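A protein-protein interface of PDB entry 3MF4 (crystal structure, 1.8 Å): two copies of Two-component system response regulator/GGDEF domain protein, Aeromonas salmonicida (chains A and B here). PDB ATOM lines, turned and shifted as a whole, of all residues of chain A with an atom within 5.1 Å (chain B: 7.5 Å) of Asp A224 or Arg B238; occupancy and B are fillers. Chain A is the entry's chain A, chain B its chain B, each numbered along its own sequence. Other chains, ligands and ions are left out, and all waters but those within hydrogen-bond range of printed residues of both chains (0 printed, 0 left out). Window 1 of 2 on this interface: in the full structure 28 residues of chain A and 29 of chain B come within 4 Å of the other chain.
CD1 of Leu A218 touches O of Glu B233, at 3.7 Å.
CB of Cys B237 touches CD1 of Leu A218, 3.8 Å away.
Asp A224 touches His B241.
CE1 of Phe A225 touches O of Glu B234, 3.5 Å away.
Phe A225 touches Cys B237.
Phe A225 touches Arg B238 (CE1 to NH1, 3.2 Å).
Asn A242 touches His B241 (OD1 to CE1, 3.97 Å).
The side-chain amide oxygen (OD1) of Asn A223 sits at hydrogen-bond distance from the backbone NH (N) of Ile A202 (2.9 Å).
The backbone NH (N) of Gly A204 is in hydrogen-bond range of the backbone carbonyl oxygen (O) of Asp A224 (2.9 Å).
The side-chain carboxylate of Asp A224 is in salt-bridge range of the guanidinium group of Arg A238, 3.8 Å away.
The side-chain carboxylate of Asp B224 lies close to the side-chain amide oxygen of Asn B242, at 3.0 Å.
The side-chain sulfur (SG) of Cys B237 sits close to a ring nitrogen (NE2) of His B241.
The backbone carbonyl oxygen (O) of Arg B238 sits close to the side-chain amide oxygen (OD1) of Asn B242, at 2.9 Å.
Hydrophobic or aromatic side chains of chain A that line the printed part of chain B: Leu A218, Phe A225 and His A241.
Along chain A the printed residues that touch a printed residue of chain B span positions 218 to 242.
Of the 23 printed residues of chain B, 7 touch a printed residue of chain A.
Hydrophobic or aromatic side chains of chain B that line the printed part of chain A: Phe B225 and His B241.
O of Asn A223 sits at hydrogen-bond distance from NE2 of His B241 (2.8 Å).
The side-chain carboxylate of Asp A224 lies within hydrogen-bond range of the side-chain sulfur of Cys B237 (3.3 Å).
The side-chain carboxylate (OD1) of Asp A224 lies within salt-bridge range of the guanidinium group (NH1) of Arg B238.
OD1 of Asp B224 is in salt-bridge range of NH2 of Arg A238 (2.8 Å).
NH2 of Arg A238 lies close to O of Phe B225.
NE2 of His A241 is in hydrogen-bond range of ND1 of His B241, 2.9 Å away.
NH1 of Arg B238 lies close to NH1 of Arg A238, 3.3 Å away.
Asn A223 touches His B241, but with the chains exchanged His A241 does not touch Asn B223 (6.7 Å).
Asp A224 touches Arg B238, and with the chains exchanged Arg A238 touches Asp B224.
His A241 touches its own counterpart, His B241.
Asn A242 touches His B241, but with the chains exchanged His A241 does not touch Asn B242 (4.8 Å).
8 positions are printed for both chains.
Of the printed residues of chain B, Leu A218 touches Glu B233 (3.7 Å) and Cys B237 (3.8 Å).
Asp A224 touches three residues of chain B.
Of the printed residues of chain B, His A241 touches His B241.
Arg B238 touches just these residues of chain A: Asp A224, Phe A225 and Arg A238.
The nearest residue of chain A that does not touch Arg B238 is His A241 (4.8 Å).
The nearest printed residue of chain A that does not touch Glu B233 is Phe A225 (5.0 Å).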
ATOM      1  N   ILE A 202     -20.334  -6.955  -4.895  1.00  0.00           N
ATOM      2  CA  ILE A 202     -20.003  -5.885  -3.996  1.00  0.00           C
ATOM      3  C   ILE A 202     -20.505  -4.609  -4.594  1.00  0.00           C
ATOM      4  O   ILE A 202     -20.163  -4.307  -5.731  1.00  0.00           O
ATOM      5  CB  ILE A 202     -18.461  -5.777  -3.752  1.00  0.00           C
ATOM      6  CG1 ILE A 202     -17.934  -7.082  -3.123  1.00  0.00           C
ATOM      7  CG2 ILE A 202     -18.160  -4.567  -2.860  1.00  0.00           C
ATOM      8  CD1 ILE A 202     -16.407  -7.239  -3.017  1.00  0.00           C
ATOM      9  N   ILE A 203     -21.325  -3.889  -3.822  1.00  0.00           N
ATOM     10  CA  ILE A 203     -21.757  -2.542  -4.169  1.00  0.00           C
ATOM     11  C   ILE A 203     -20.975  -1.563  -3.270  1.00  0.00           C
ATOM     12  O   ILE A 203     -21.030  -1.632  -2.052  1.00  0.00           O
ATOM     13  CB  ILE A 203     -23.295  -2.375  -4.033  1.00  0.00           C
ATOM     14  CG1 ILE A 203     -24.031  -3.222  -5.085  1.00  0.00           C
ATOM     15  CG2 ILE A 203     -23.701  -0.904  -4.167  1.00  0.00           C
ATOM     16  CD1 ILE A 203     -25.590  -3.248  -4.929  1.00  0.00           C
ATOM     17  N   GLY A 204     -20.223  -0.664  -3.888  1.00  0.00           N
ATOM     18  CA  GLY A 204     -19.477   0.344  -3.143  1.00  0.00           C
ATOM     19  C   GLY A 204     -20.323   1.575  -2.869  1.00  0.00           C
ATOM     20  O   GLY A 204     -20.854   2.196  -3.796  1.00  0.00           O
ATOM     21  N   LEU A 218     -14.698   0.544  -8.694  1.00  0.00           N
ATOM     22  CA  LEU A 218     -14.892  -0.293  -9.892  1.00  0.00           C
ATOM     23  C   LEU A 218     -13.578  -0.863 -10.384  1.00  0.00           C
ATOM     24  O   LEU A 218     -13.497  -2.048 -10.713  1.00  0.00           O
ATOM     25  CB  LEU A 218     -15.587   0.487 -11.024  1.00  0.00           C
ATOM     26  CG  LEU A 218     -16.965   0.999 -10.575  1.00  0.00           C
ATOM     27  CD1 LEU A 218     -17.474   2.097 -11.512  1.00  0.00           C
ATOM     28  CD2 LEU A 218     -17.949  -0.129 -10.408  1.00  0.00           C
ATOM     29  N   ALA A 222     -15.339  -3.849  -7.576  1.00  0.00           N
ATOM     30  CA  ALA A 222     -16.716  -3.709  -7.130  1.00  0.00           C
ATOM     31  C   ALA A 222     -17.608  -3.894  -8.345  1.00  0.00           C
ATOM     32  O   ALA A 222     -17.328  -3.358  -9.418  1.00  0.00           O
ATOM     33  CB  ALA A 222     -16.971  -2.342  -6.490  1.00  0.00           C
ATOM     34  N   ASN A 223     -18.677  -4.657  -8.175  1.00  0.00           N
ATOM     35  CA  ASN A 223     -19.695  -4.816  -9.228  1.00  0.00           C
ATOM     36  C   ASN A 223     -20.370  -3.528  -9.627  1.00  0.00           C
ATOM     37  O   ASN A 223     -20.721  -3.330 -10.789  1.00  0.00           O
ATOM     38  CB  ASN A 223     -20.787  -5.755  -8.740  1.00  0.00           C
ATOM     39  CG  ASN A 223     -20.267  -7.131  -8.502  1.00  0.00           C
ATOM     40  OD1 ASN A 223     -19.454  -7.341  -7.605  1.00  0.00           O
ATOM     41  ND2 ASN A 223     -20.684  -8.077  -9.341  1.00  0.00           N
ATOM     42  N   ASP A 224     -20.582  -2.667  -8.641  1.00  0.00           N
ATOM     43  CA  ASP A 224     -21.405  -1.477  -8.851  1.00  0.00           C
ATOM     44  C   ASP A 224     -21.139  -0.422  -7.777  1.00  0.00           C
ATOM     45  O   ASP A 224     -20.396  -0.674  -6.819  1.00  0.00           O
ATOM     46  CB  ASP A 224     -22.898  -1.887  -8.856  1.00  0.00           C
ATOM     47  CG  ASP A 224     -23.729  -1.033  -9.788  1.00  0.00           C
ATOM     48  OD1 ASP A 224     -23.230   0.046 -10.195  1.00  0.00           O
ATOM     49  OD2 ASP A 224     -24.870  -1.445 -10.127  1.00  0.00           O
ATOM     50  N   PHE A 225     -21.728   0.758  -7.966  1.00  0.00           N
ATOM     51  CA  PHE A 225     -21.645   1.848  -7.010  1.00  0.00           C
ATOM     52  C   PHE A 225     -23.044   2.348  -6.656  1.00  0.00           C
ATOM     53  O   PHE A 225     -24.009   2.167  -7.416  1.00  0.00           O
ATOM     54  CB  PHE A 225     -20.829   3.025  -7.602  1.00  0.00           C
ATOM     55  CG  PHE A 225     -21.538   3.728  -8.715  1.00  0.00           C
ATOM     56  CD1 PHE A 225     -21.523   3.211 -10.005  1.00  0.00           C
ATOM     57  CD2 PHE A 225     -22.273   4.885  -8.467  1.00  0.00           C
ATOM     58  CE1 PHE A 225     -22.222   3.855 -11.038  1.00  0.00           C
ATOM     59  CE2 PHE A 225     -22.965   5.527  -9.482  1.00  0.00           C
ATOM     60  CZ  PHE A 225     -22.955   5.008 -10.761  1.00  0.00           C
ATOM     61  N   LEU A 226     -23.141   2.993  -5.502  1.00  0.00           N
ATOM     62  CA  LEU A 226     -24.362   3.703  -5.087  1.00  0.00           C
ATOM     63  C   LEU A 226     -23.957   4.931  -4.266  1.00  0.00           C
ATOM     64  O   LEU A 226     -23.270   4.804  -3.251  1.00  0.00           O
ATOM     65  CB  LEU A 226     -25.277   2.787  -4.273  1.00  0.00           C
ATOM     66  CG  LEU A 226     -26.600   3.368  -3.752  1.00  0.00           C
ATOM     67  CD1 LEU A 226     -27.568   3.540  -4.899  1.00  0.00           C
ATOM     68  CD2 LEU A 226     -27.166   2.375  -2.732  1.00  0.00           C
ATOM     69  N   ARG A 238     -30.765  -0.728  -7.527  1.00  0.00           N
ATOM     70  CA  ARG A 238     -29.346  -1.082  -7.632  1.00  0.00           C
ATOM     71  C   ARG A 238     -29.099  -2.480  -7.064  1.00  0.00           C
ATOM     72  O   ARG A 238     -28.346  -3.262  -7.655  1.00  0.00           O
ATOM     73  CB  ARG A 238     -28.511  -0.044  -6.867  1.00  0.00           C
ATOM     74  CG  ARG A 238     -27.003  -0.070  -7.088  1.00  0.00           C
ATOM     75  CD  ARG A 238     -26.533   0.400  -8.486  1.00  0.00           C
ATOM     76  NE  ARG A 238     -27.489   1.154  -9.290  1.00  0.00           N
ATOM     77  CZ  ARG A 238     -27.424   2.466  -9.512  1.00  0.00           C
ATOM     78  NH1 ARG A 238     -26.448   3.197  -8.974  1.00  0.00           N
ATOM     79  NH2 ARG A 238     -28.328   3.039 -10.275  1.00  0.00           N
ATOM     80  N   HIS A 241     -30.733  -5.210  -9.429  1.00  0.00           N
ATOM     81  CA  HIS A 241     -29.970  -5.454 -10.616  1.00  0.00           C
ATOM     82  C   HIS A 241     -28.797  -6.395 -10.342  1.00  0.00           C
ATOM     83  O   HIS A 241     -28.554  -7.331 -11.106  1.00  0.00           O
ATOM     84  CB  HIS A 241     -29.446  -4.160 -11.260  1.00  0.00           C
ATOM     85  CG  HIS A 241     -28.502  -4.417 -12.390  1.00  0.00           C
ATOM     86  ND1 HIS A 241     -28.933  -4.693 -13.672  1.00  0.00           N
ATOM     87  CD2 HIS A 241     -27.151  -4.516 -12.417  1.00  0.00           C
ATOM     88  CE1 HIS A 241     -27.886  -4.910 -14.446  1.00  0.00           C
ATOM     89  NE2 HIS A 241     -26.792  -4.820 -13.708  1.00  0.00           N
ATOM     90  N   ASN A 242     -28.067  -6.125  -9.261  1.00  0.00           N
ATOM     91  CA  ASN A 242     -26.876  -6.883  -8.965  1.00  0.00           C
ATOM     92  C   ASN A 242     -27.176  -8.290  -8.539  1.00  0.00           C
ATOM     93  O   ASN A 242     -26.417  -9.224  -8.853  1.00  0.00           O
ATOM     94  CB  ASN A 242     -26.013  -6.137  -7.951  1.00  0.00           C
ATOM     95  CG  ASN A 242     -25.254  -5.018  -8.613  1.00  0.00           C
ATOM     96  OD1 ASN A 242     -24.239  -5.255  -9.290  1.00  0.00           O
ATOM     97  ND2 ASN A 242     -25.769  -3.818  -8.512  1.00  0.00           N
ATOM     98  N   GLN B 147     -16.910   4.812 -24.997  1.00  0.00           N
ATOM     99  CA  GLN B 147     -17.233   3.420 -24.711  1.00  0.00           C
ATOM    100  C   GLN B 147     -17.423   2.676 -26.064  1.00  0.00           C
ATOM    101  O   GLN B 147     -17.855   1.526 -26.090  1.00  0.00           O
ATOM    102  CB  GLN B 147     -18.495   3.330 -23.838  1.00  0.00           C
ATOM    103  CG  GLN B 147     -18.422   4.091 -22.512  1.00  0.00           C
ATOM    104  CD  GLN B 147     -19.756   4.136 -21.780  1.00  0.00           C
ATOM    105  OE1 GLN B 147     -20.502   3.148 -21.745  1.00  0.00           O
ATOM    106  NE2 GLN B 147     -20.058   5.285 -21.176  1.00  0.00           N
ATOM    107  N   LEU B 172     -31.001   1.877 -26.199  1.00  0.00           N
ATOM    108  CA  LEU B 172     -30.856   2.561 -24.895  1.00  0.00           C
ATOM    109  C   LEU B 172     -30.951   4.076 -25.013  1.00  0.00           C
ATOM    110  O   LEU B 172     -30.242   4.692 -25.813  1.00  0.00           O
ATOM    111  CB  LEU B 172     -29.559   2.167 -24.186  1.00  0.00           C
ATOM    112  CG  LEU B 172     -29.170   3.078 -23.000  1.00  0.00           C
ATOM    113  CD1 LEU B 172     -29.912   2.645 -21.743  1.00  0.00           C
ATOM    114  CD2 LEU B 172     -27.650   3.066 -22.786  1.00  0.00           C
ATOM    115  N   LEU B 174     -30.918   7.728 -22.807  1.00  0.00           N
ATOM    116  CA  LEU B 174     -30.624   8.422 -21.564  1.00  0.00           C
ATOM    117  C   LEU B 174     -31.394   9.723 -21.607  1.00  0.00           C
ATOM    118  O   LEU B 174     -31.194  10.514 -22.527  1.00  0.00           O
ATOM    119  CB  LEU B 174     -29.117   8.670 -21.451  1.00  0.00           C
ATOM    120  CG  LEU B 174     -28.235   7.425 -21.259  1.00  0.00           C
ATOM    121  CD1 LEU B 174     -27.869   6.808 -22.602  1.00  0.00           C
ATOM    122  CD2 LEU B 174     -26.953   7.832 -20.549  1.00  0.00           C
ATOM    123  N   ILE B 203     -32.456   4.974 -19.097  1.00  0.00           N
ATOM    124  CA  ILE B 203     -31.803   5.521 -17.892  1.00  0.00           C
ATOM    125  C   ILE B 203     -32.245   6.957 -17.683  1.00  0.00           C
ATOM    126  O   ILE B 203     -31.992   7.839 -18.536  1.00  0.00           O
ATOM    127  CB  ILE B 203     -30.243   5.465 -17.952  1.00  0.00           C
ATOM    128  CG1 ILE B 203     -29.748   4.031 -18.199  1.00  0.00           C
ATOM    129  CG2 ILE B 203     -29.655   6.096 -16.670  1.00  0.00           C
ATOM    130  CD1 ILE B 203     -28.252   3.927 -18.551  1.00  0.00           C
ATOM    131  N   ASN B 223     -35.462   1.870 -16.671  1.00  0.00           N
ATOM    132  CA  ASN B 223     -34.684   0.711 -16.218  1.00  0.00           C
ATOM    133  C   ASN B 223     -33.800   1.129 -15.051  1.00  0.00           C
ATOM    134  O   ASN B 223     -33.522   0.344 -14.156  1.00  0.00           O
ATOM    135  CB  ASN B 223     -33.769   0.189 -17.338  1.00  0.00           C
ATOM    136  CG  ASN B 223     -34.537  -0.361 -18.525  1.00  0.00           C
ATOM    137  OD1 ASN B 223     -35.108   0.389 -19.292  1.00  0.00           O
ATOM    138  ND2 ASN B 223     -34.526  -1.677 -18.690  1.00  0.00           N
ATOM    139  N   ASP B 224     -33.357   2.377 -15.073  1.00  0.00           N
ATOM    140  CA  ASP B 224     -32.295   2.795 -14.172  1.00  0.00           C
ATOM    141  C   ASP B 224     -32.262   4.307 -14.033  1.00  0.00           C
ATOM    142  O   ASP B 224     -32.975   5.030 -14.737  1.00  0.00           O
ATOM    143  CB  ASP B 224     -30.953   2.252 -14.699  1.00  0.00           C
ATOM    144  CG  ASP B 224     -29.912   1.986 -13.594  1.00  0.00           C
ATOM    145  OD1 ASP B 224     -30.044   2.448 -12.449  1.00  0.00           O
ATOM    146  OD2 ASP B 224     -28.898   1.329 -13.905  1.00  0.00           O
ATOM    147  N   PHE B 225     -31.435   4.762 -13.102  1.00  0.00           N
ATOM    148  CA  PHE B 225     -31.265   6.173 -12.821  1.00  0.00           C
ATOM    149  C   PHE B 225     -29.784   6.494 -12.746  1.00  0.00           C
ATOM    150  O   PHE B 225     -28.961   5.648 -12.405  1.00  0.00           O
ATOM    151  CB  PHE B 225     -31.914   6.510 -11.462  1.00  0.00           C
ATOM    152  CG  PHE B 225     -31.159   5.948 -10.288  1.00  0.00           C
ATOM    153  CD1 PHE B 225     -30.177   6.701  -9.644  1.00  0.00           C
ATOM    154  CD2 PHE B 225     -31.450   4.669  -9.810  1.00  0.00           C
ATOM    155  CE1 PHE B 225     -29.471   6.178  -8.575  1.00  0.00           C
ATOM    156  CE2 PHE B 225     -30.738   4.139  -8.736  1.00  0.00           C
ATOM    157  CZ  PHE B 225     -29.763   4.903  -8.110  1.00  0.00           C
ATOM    158  N   LEU B 226     -29.441   7.734 -13.059  1.00  0.00           N
ATOM    159  CA  LEU B 226     -28.096   8.207 -12.829  1.00  0.00           C
ATOM    160  C   LEU B 226     -28.238   9.648 -12.412  1.00  0.00           C
ATOM    161  O   LEU B 226     -28.882  10.423 -13.108  1.00  0.00           O
ATOM    162  CB  LEU B 226     -27.240   8.048 -14.096  1.00  0.00           C
ATOM    163  CG  LEU B 226     -25.747   8.408 -14.041  1.00  0.00           C
ATOM    164  CD1 LEU B 226     -25.017   7.656 -12.950  1.00  0.00           C
ATOM    165  CD2 LEU B 226     -25.104   8.123 -15.380  1.00  0.00           C
ATOM    166  N   ASN B 227     -27.675  10.000 -11.256  1.00  0.00           N
ATOM    167  CA  ASN B 227     -27.796  11.357 -10.749  1.00  0.00           C
ATOM    168  C   ASN B 227     -26.640  12.252 -11.204  1.00  0.00           C
ATOM    169  O   ASN B 227     -25.469  11.857 -11.131  1.00  0.00           O
ATOM    170  CB  ASN B 227     -27.958  11.374  -9.219  1.00  0.00           C
ATOM    171  CG  ASN B 227     -29.213  10.634  -8.747  1.00  0.00           C
ATOM    172  OD1 ASN B 227     -30.317  10.827  -9.289  1.00  0.00           O
ATOM    173  ND2 ASN B 227     -29.046   9.771  -7.736  1.00  0.00           N
ATOM    174  N   PHE B 230     -22.170  13.364 -12.473  1.00  0.00           N
ATOM    175  CA  PHE B 230     -21.579  12.028 -12.452  1.00  0.00           C
ATOM    176  C   PHE B 230     -20.250  12.009 -13.194  1.00  0.00           C
ATOM    177  O   PHE B 230     -20.010  12.839 -14.085  1.00  0.00           O
ATOM    178  CB  PHE B 230     -22.537  10.971 -13.052  1.00  0.00           C
ATOM    179  CG  PHE B 230     -23.027  11.296 -14.449  1.00  0.00           C
ATOM    180  CD1 PHE B 230     -22.242  11.005 -15.570  1.00  0.00           C
ATOM    181  CD2 PHE B 230     -24.287  11.867 -14.643  1.00  0.00           C
ATOM    182  CE1 PHE B 230     -22.697  11.300 -16.861  1.00  0.00           C
ATOM    183  CE2 PHE B 230     -24.747  12.171 -15.933  1.00  0.00           C
ATOM    184  CZ  PHE B 230     -23.949  11.884 -17.040  1.00  0.00           C
ATOM    185  N   PRO B 232     -17.178   9.881 -15.505  1.00  0.00           N
ATOM    186  CA  PRO B 232     -17.283   8.992 -16.661  1.00  0.00           C
ATOM    187  C   PRO B 232     -17.385   7.516 -16.293  1.00  0.00           C
ATOM    188  O   PRO B 232     -18.118   6.771 -16.946  1.00  0.00           O
ATOM    189  CB  PRO B 232     -15.980   9.243 -17.419  1.00  0.00           C
ATOM    190  CG  PRO B 232     -15.545  10.588 -16.984  1.00  0.00           C
ATOM    191  CD  PRO B 232     -15.931  10.676 -15.559  1.00  0.00           C
ATOM    192  N   GLU B 233     -16.664   7.103 -15.256  1.00  0.00           N
ATOM    193  CA  GLU B 233     -16.703   5.722 -14.813  1.00  0.00           C
ATOM    194  C   GLU B 233     -18.072   5.361 -14.287  1.00  0.00           C
ATOM    195  O   GLU B 233     -18.464   4.199 -14.359  1.00  0.00           O
ATOM    196  CB  GLU B 233     -15.631   5.436 -13.754  1.00  0.00           C
ATOM    197  CG  GLU B 233     -14.173   5.727 -14.231  1.00  0.00           C
ATOM    198  CD  GLU B 233     -13.745   7.184 -14.020  1.00  0.00           C
ATOM    199  OE1 GLU B 233     -14.613   8.050 -13.804  1.00  0.00           O
ATOM    200  OE2 GLU B 233     -12.522   7.465 -14.046  1.00  0.00           O
ATOM    201  N   GLU B 234     -18.781   6.342 -13.732  1.00  0.00           N
ATOM    202  CA  GLU B 234     -20.146   6.128 -13.273  1.00  0.00           C
ATOM    203  C   GLU B 234     -21.119   5.853 -14.417  1.00  0.00           C
ATOM    204  O   GLU B 234     -21.885   4.888 -14.360  1.00  0.00           O
ATOM    205  CB  GLU B 234     -20.612   7.264 -12.375  1.00  0.00           C
ATOM    206  CG  GLU B 234     -19.967   7.155 -11.008  1.00  0.00           C
ATOM    207  CD  GLU B 234     -20.198   8.372 -10.125  1.00  0.00           C
ATOM    208  OE1 GLU B 234     -20.233   8.182  -8.892  1.00  0.00           O
ATOM    209  OE2 GLU B 234     -20.306   9.498 -10.656  1.00  0.00           O
ATOM    210  N   LEU B 235     -21.061   6.694 -15.445  1.00  0.00           N
ATOM    211  CA  LEU B 235     -21.839   6.510 -16.669  1.00  0.00           C
ATOM    212  C   LEU B 235     -21.484   5.185 -17.345  1.00  0.00           C
ATOM    213  O   LEU B 235     -22.377   4.419 -17.731  1.00  0.00           O
ATOM    214  CB  LEU B 235     -21.599   7.692 -17.641  1.00  0.00           C
ATOM    215  CG  LEU B 235     -22.339   7.630 -18.992  1.00  0.00           C
ATOM    216  CD1 LEU B 235     -23.781   7.905 -18.697  1.00  0.00           C
ATOM    217  CD2 LEU B 235     -21.753   8.681 -19.973  1.00  0.00           C
ATOM    218  N   GLN B 236     -20.184   4.904 -17.481  1.00  0.00           N
ATOM    219  CA  GLN B 236     -19.750   3.656 -18.114  1.00  0.00           C
ATOM    220  C   GLN B 236     -20.321   2.443 -17.382  1.00  0.00           C
ATOM    221  O   GLN B 236     -20.896   1.547 -18.003  1.00  0.00           O
ATOM    222  CB  GLN B 236     -18.225   3.560 -18.197  1.00  0.00           C
ATOM    223  CG  GLN B 236     -17.747   2.278 -18.862  1.00  0.00           C
ATOM    224  CD  GLN B 236     -16.271   2.294 -19.233  1.00  0.00           C
ATOM    225  OE1 GLN B 236     -15.917   2.085 -20.400  1.00  0.00           O
ATOM    226  NE2 GLN B 236     -15.402   2.513 -18.244  1.00  0.00           N
ATOM    227  N   CYS B 237     -20.164   2.435 -16.066  1.00  0.00           N
ATOM    228  CA  CYS B 237     -20.731   1.380 -15.226  1.00  0.00           C
ATOM    229  C   CYS B 237     -22.228   1.198 -15.474  1.00  0.00           C
ATOM    230  O   CYS B 237     -22.682   0.092 -15.783  1.00  0.00           O
ATOM    231  CB  CYS B 237     -20.503   1.712 -13.762  1.00  0.00           C
ATOM    232  SG  CYS B 237     -21.071   0.403 -12.698  1.00  0.00           S
ATOM    233  N   ARG B 238     -22.985   2.290 -15.334  1.00  0.00           N
ATOM    234  CA  ARG B 238     -24.440   2.252 -15.532  1.00  0.00           C
ATOM    235  C   ARG B 238     -24.830   1.769 -16.937  1.00  0.00           C
ATOM    236  O   ARG B 238     -25.632   0.867 -17.081  1.00  0.00           O
ATOM    237  CB  ARG B 238     -25.063   3.628 -15.276  1.00  0.00           C
ATOM    238  CG  ARG B 238     -25.098   4.065 -13.834  1.00  0.00           C
ATOM    239  CD  ARG B 238     -26.402   3.652 -13.126  1.00  0.00           C
ATOM    240  NE  ARG B 238     -26.550   2.202 -12.995  1.00  0.00           N
ATOM    241  CZ  ARG B 238     -25.766   1.427 -12.252  1.00  0.00           C
ATOM    242  NH1 ARG B 238     -24.763   1.954 -11.560  1.00  0.00           N
ATOM    243  NH2 ARG B 238     -25.987   0.123 -12.198  1.00  0.00           N
ATOM    244  N   VAL B 239     -24.266   2.388 -17.970  1.00  0.00           N
ATOM    245  CA  VAL B 239     -24.592   1.989 -19.324  1.00  0.00           C
ATOM    246  C   VAL B 239     -24.256   0.513 -19.542  1.00  0.00           C
ATOM    247  O   VAL B 239     -25.064  -0.213 -20.117  1.00  0.00           O
ATOM    248  CB  VAL B 239     -23.941   2.933 -20.359  1.00  0.00           C
ATOM    249  CG1 VAL B 239     -24.097   2.363 -21.771  1.00  0.00           C
ATOM    250  CG2 VAL B 239     -24.577   4.316 -20.221  1.00  0.00           C
ATOM    251  N   SER B 240     -23.096   0.066 -19.040  1.00  0.00           N
ATOM    252  CA  SER B 240     -22.647  -1.321 -19.221  1.00  0.00           C
ATOM    253  C   SER B 240     -23.635  -2.299 -18.591  1.00  0.00           C
ATOM    254  O   SER B 240     -24.027  -3.276 -19.234  1.00  0.00           O
ATOM    255  CB  SER B 240     -21.214  -1.548 -18.686  1.00  0.00           C
ATOM    256  OG  SER B 240     -20.248  -0.899 -19.528  1.00  0.00           O
ATOM    257  N   HIS B 241     -24.067  -1.999 -17.358  1.00  0.00           N
ATOM    258  CA  HIS B 241     -25.030  -2.839 -16.633  1.00  0.00           C
ATOM    259  C   HIS B 241     -26.346  -2.958 -17.407  1.00  0.00           C
ATOM    260  O   HIS B 241     -26.911  -4.034 -17.509  1.00  0.00           O
ATOM    261  CB  HIS B 241     -25.319  -2.273 -15.236  1.00  0.00           C
ATOM    262  CG  HIS B 241     -24.291  -2.637 -14.209  1.00  0.00           C
ATOM    263  ND1 HIS B 241     -24.080  -3.934 -13.796  1.00  0.00           N
ATOM    264  CD2 HIS B 241     -23.429  -1.873 -13.497  1.00  0.00           C
ATOM    265  CE1 HIS B 241     -23.129  -3.955 -12.875  1.00  0.00           C
ATOM    266  NE2 HIS B 241     -22.715  -2.717 -12.682  1.00  0.00           N
ATOM    267  N   ASN B 242     -26.817  -1.851 -17.952  1.00  0.00           N
ATOM    268  CA  ASN B 242     -28.065  -1.870 -18.713  1.00  0.00           C
ATOM    269  C   ASN B 242     -27.967  -2.626 -20.028  1.00  0.00           C
ATOM    270  O   ASN B 242     -28.871  -3.380 -20.356  1.00  0.00           O
ATOM    271  CB  ASN B 242     -28.649  -0.473 -18.870  1.00  0.00           C
ATOM    272  CG  ASN B 242     -29.218   0.039 -17.578  1.00  0.00           C
ATOM    273  OD1 ASN B 242     -28.495   0.589 -16.758  1.00  0.00           O
ATOM    274  ND2 ASN B 242     -30.503  -0.192 -17.355  1.00  0.00           N
ATOM    275  N   LEU B 243     -26.854  -2.464 -20.734  1.00  0.00           N
ATOM    276  CA  LEU B 243     -26.618  -3.195 -21.967  1.00  0.00           C
ATOM    277  C   LEU B 243     -26.504  -4.700 -21.687  1.00  0.00           C
ATOM    278  O   LEU B 243     -27.076  -5.504 -22.396  1.00  0.00           O
ATOM    279  CB  LEU B 243     -25.406  -2.650 -22.709  1.00  0.00           C
ATOM    280  CG  LEU B 243     -25.617  -1.245 -23.288  1.00  0.00           C
ATOM    281  CD1 LEU B 243     -24.376  -0.712 -23.897  1.00  0.00           C
ATOM    282  CD2 LEU B 243     -26.771  -1.198 -24.301  1.00  0.00           C
ATOM    283  N   GLU B 244     -25.797  -5.060 -20.628  1.00  0.00           N
ATOM    284  CA  GLU B 244     -25.686  -6.450 -20.209  1.00  0.00           C
ATOM    285  C   GLU B 244     -27.064  -7.011 -19.836  1.00  0.00           C
ATOM    286  O   GLU B 244     -27.386  -8.140 -20.197  1.00  0.00           O
ATOM    287  CB  GLU B 244     -24.658  -6.581 -19.064  1.00  0.00           C
ATOM    288  CG  GLU B 244     -24.740  -7.871 -18.256  1.00  0.00           C
ATOM    289  CD  GLU B 244     -23.788  -8.955 -18.738  1.00  0.00           C
ATOM    290  OE1 GLU B 244     -23.539  -9.905 -17.956  1.00  0.00           O
ATOM    291  OE2 GLU B 244     -23.294  -8.881 -19.888  1.00  0.00           O
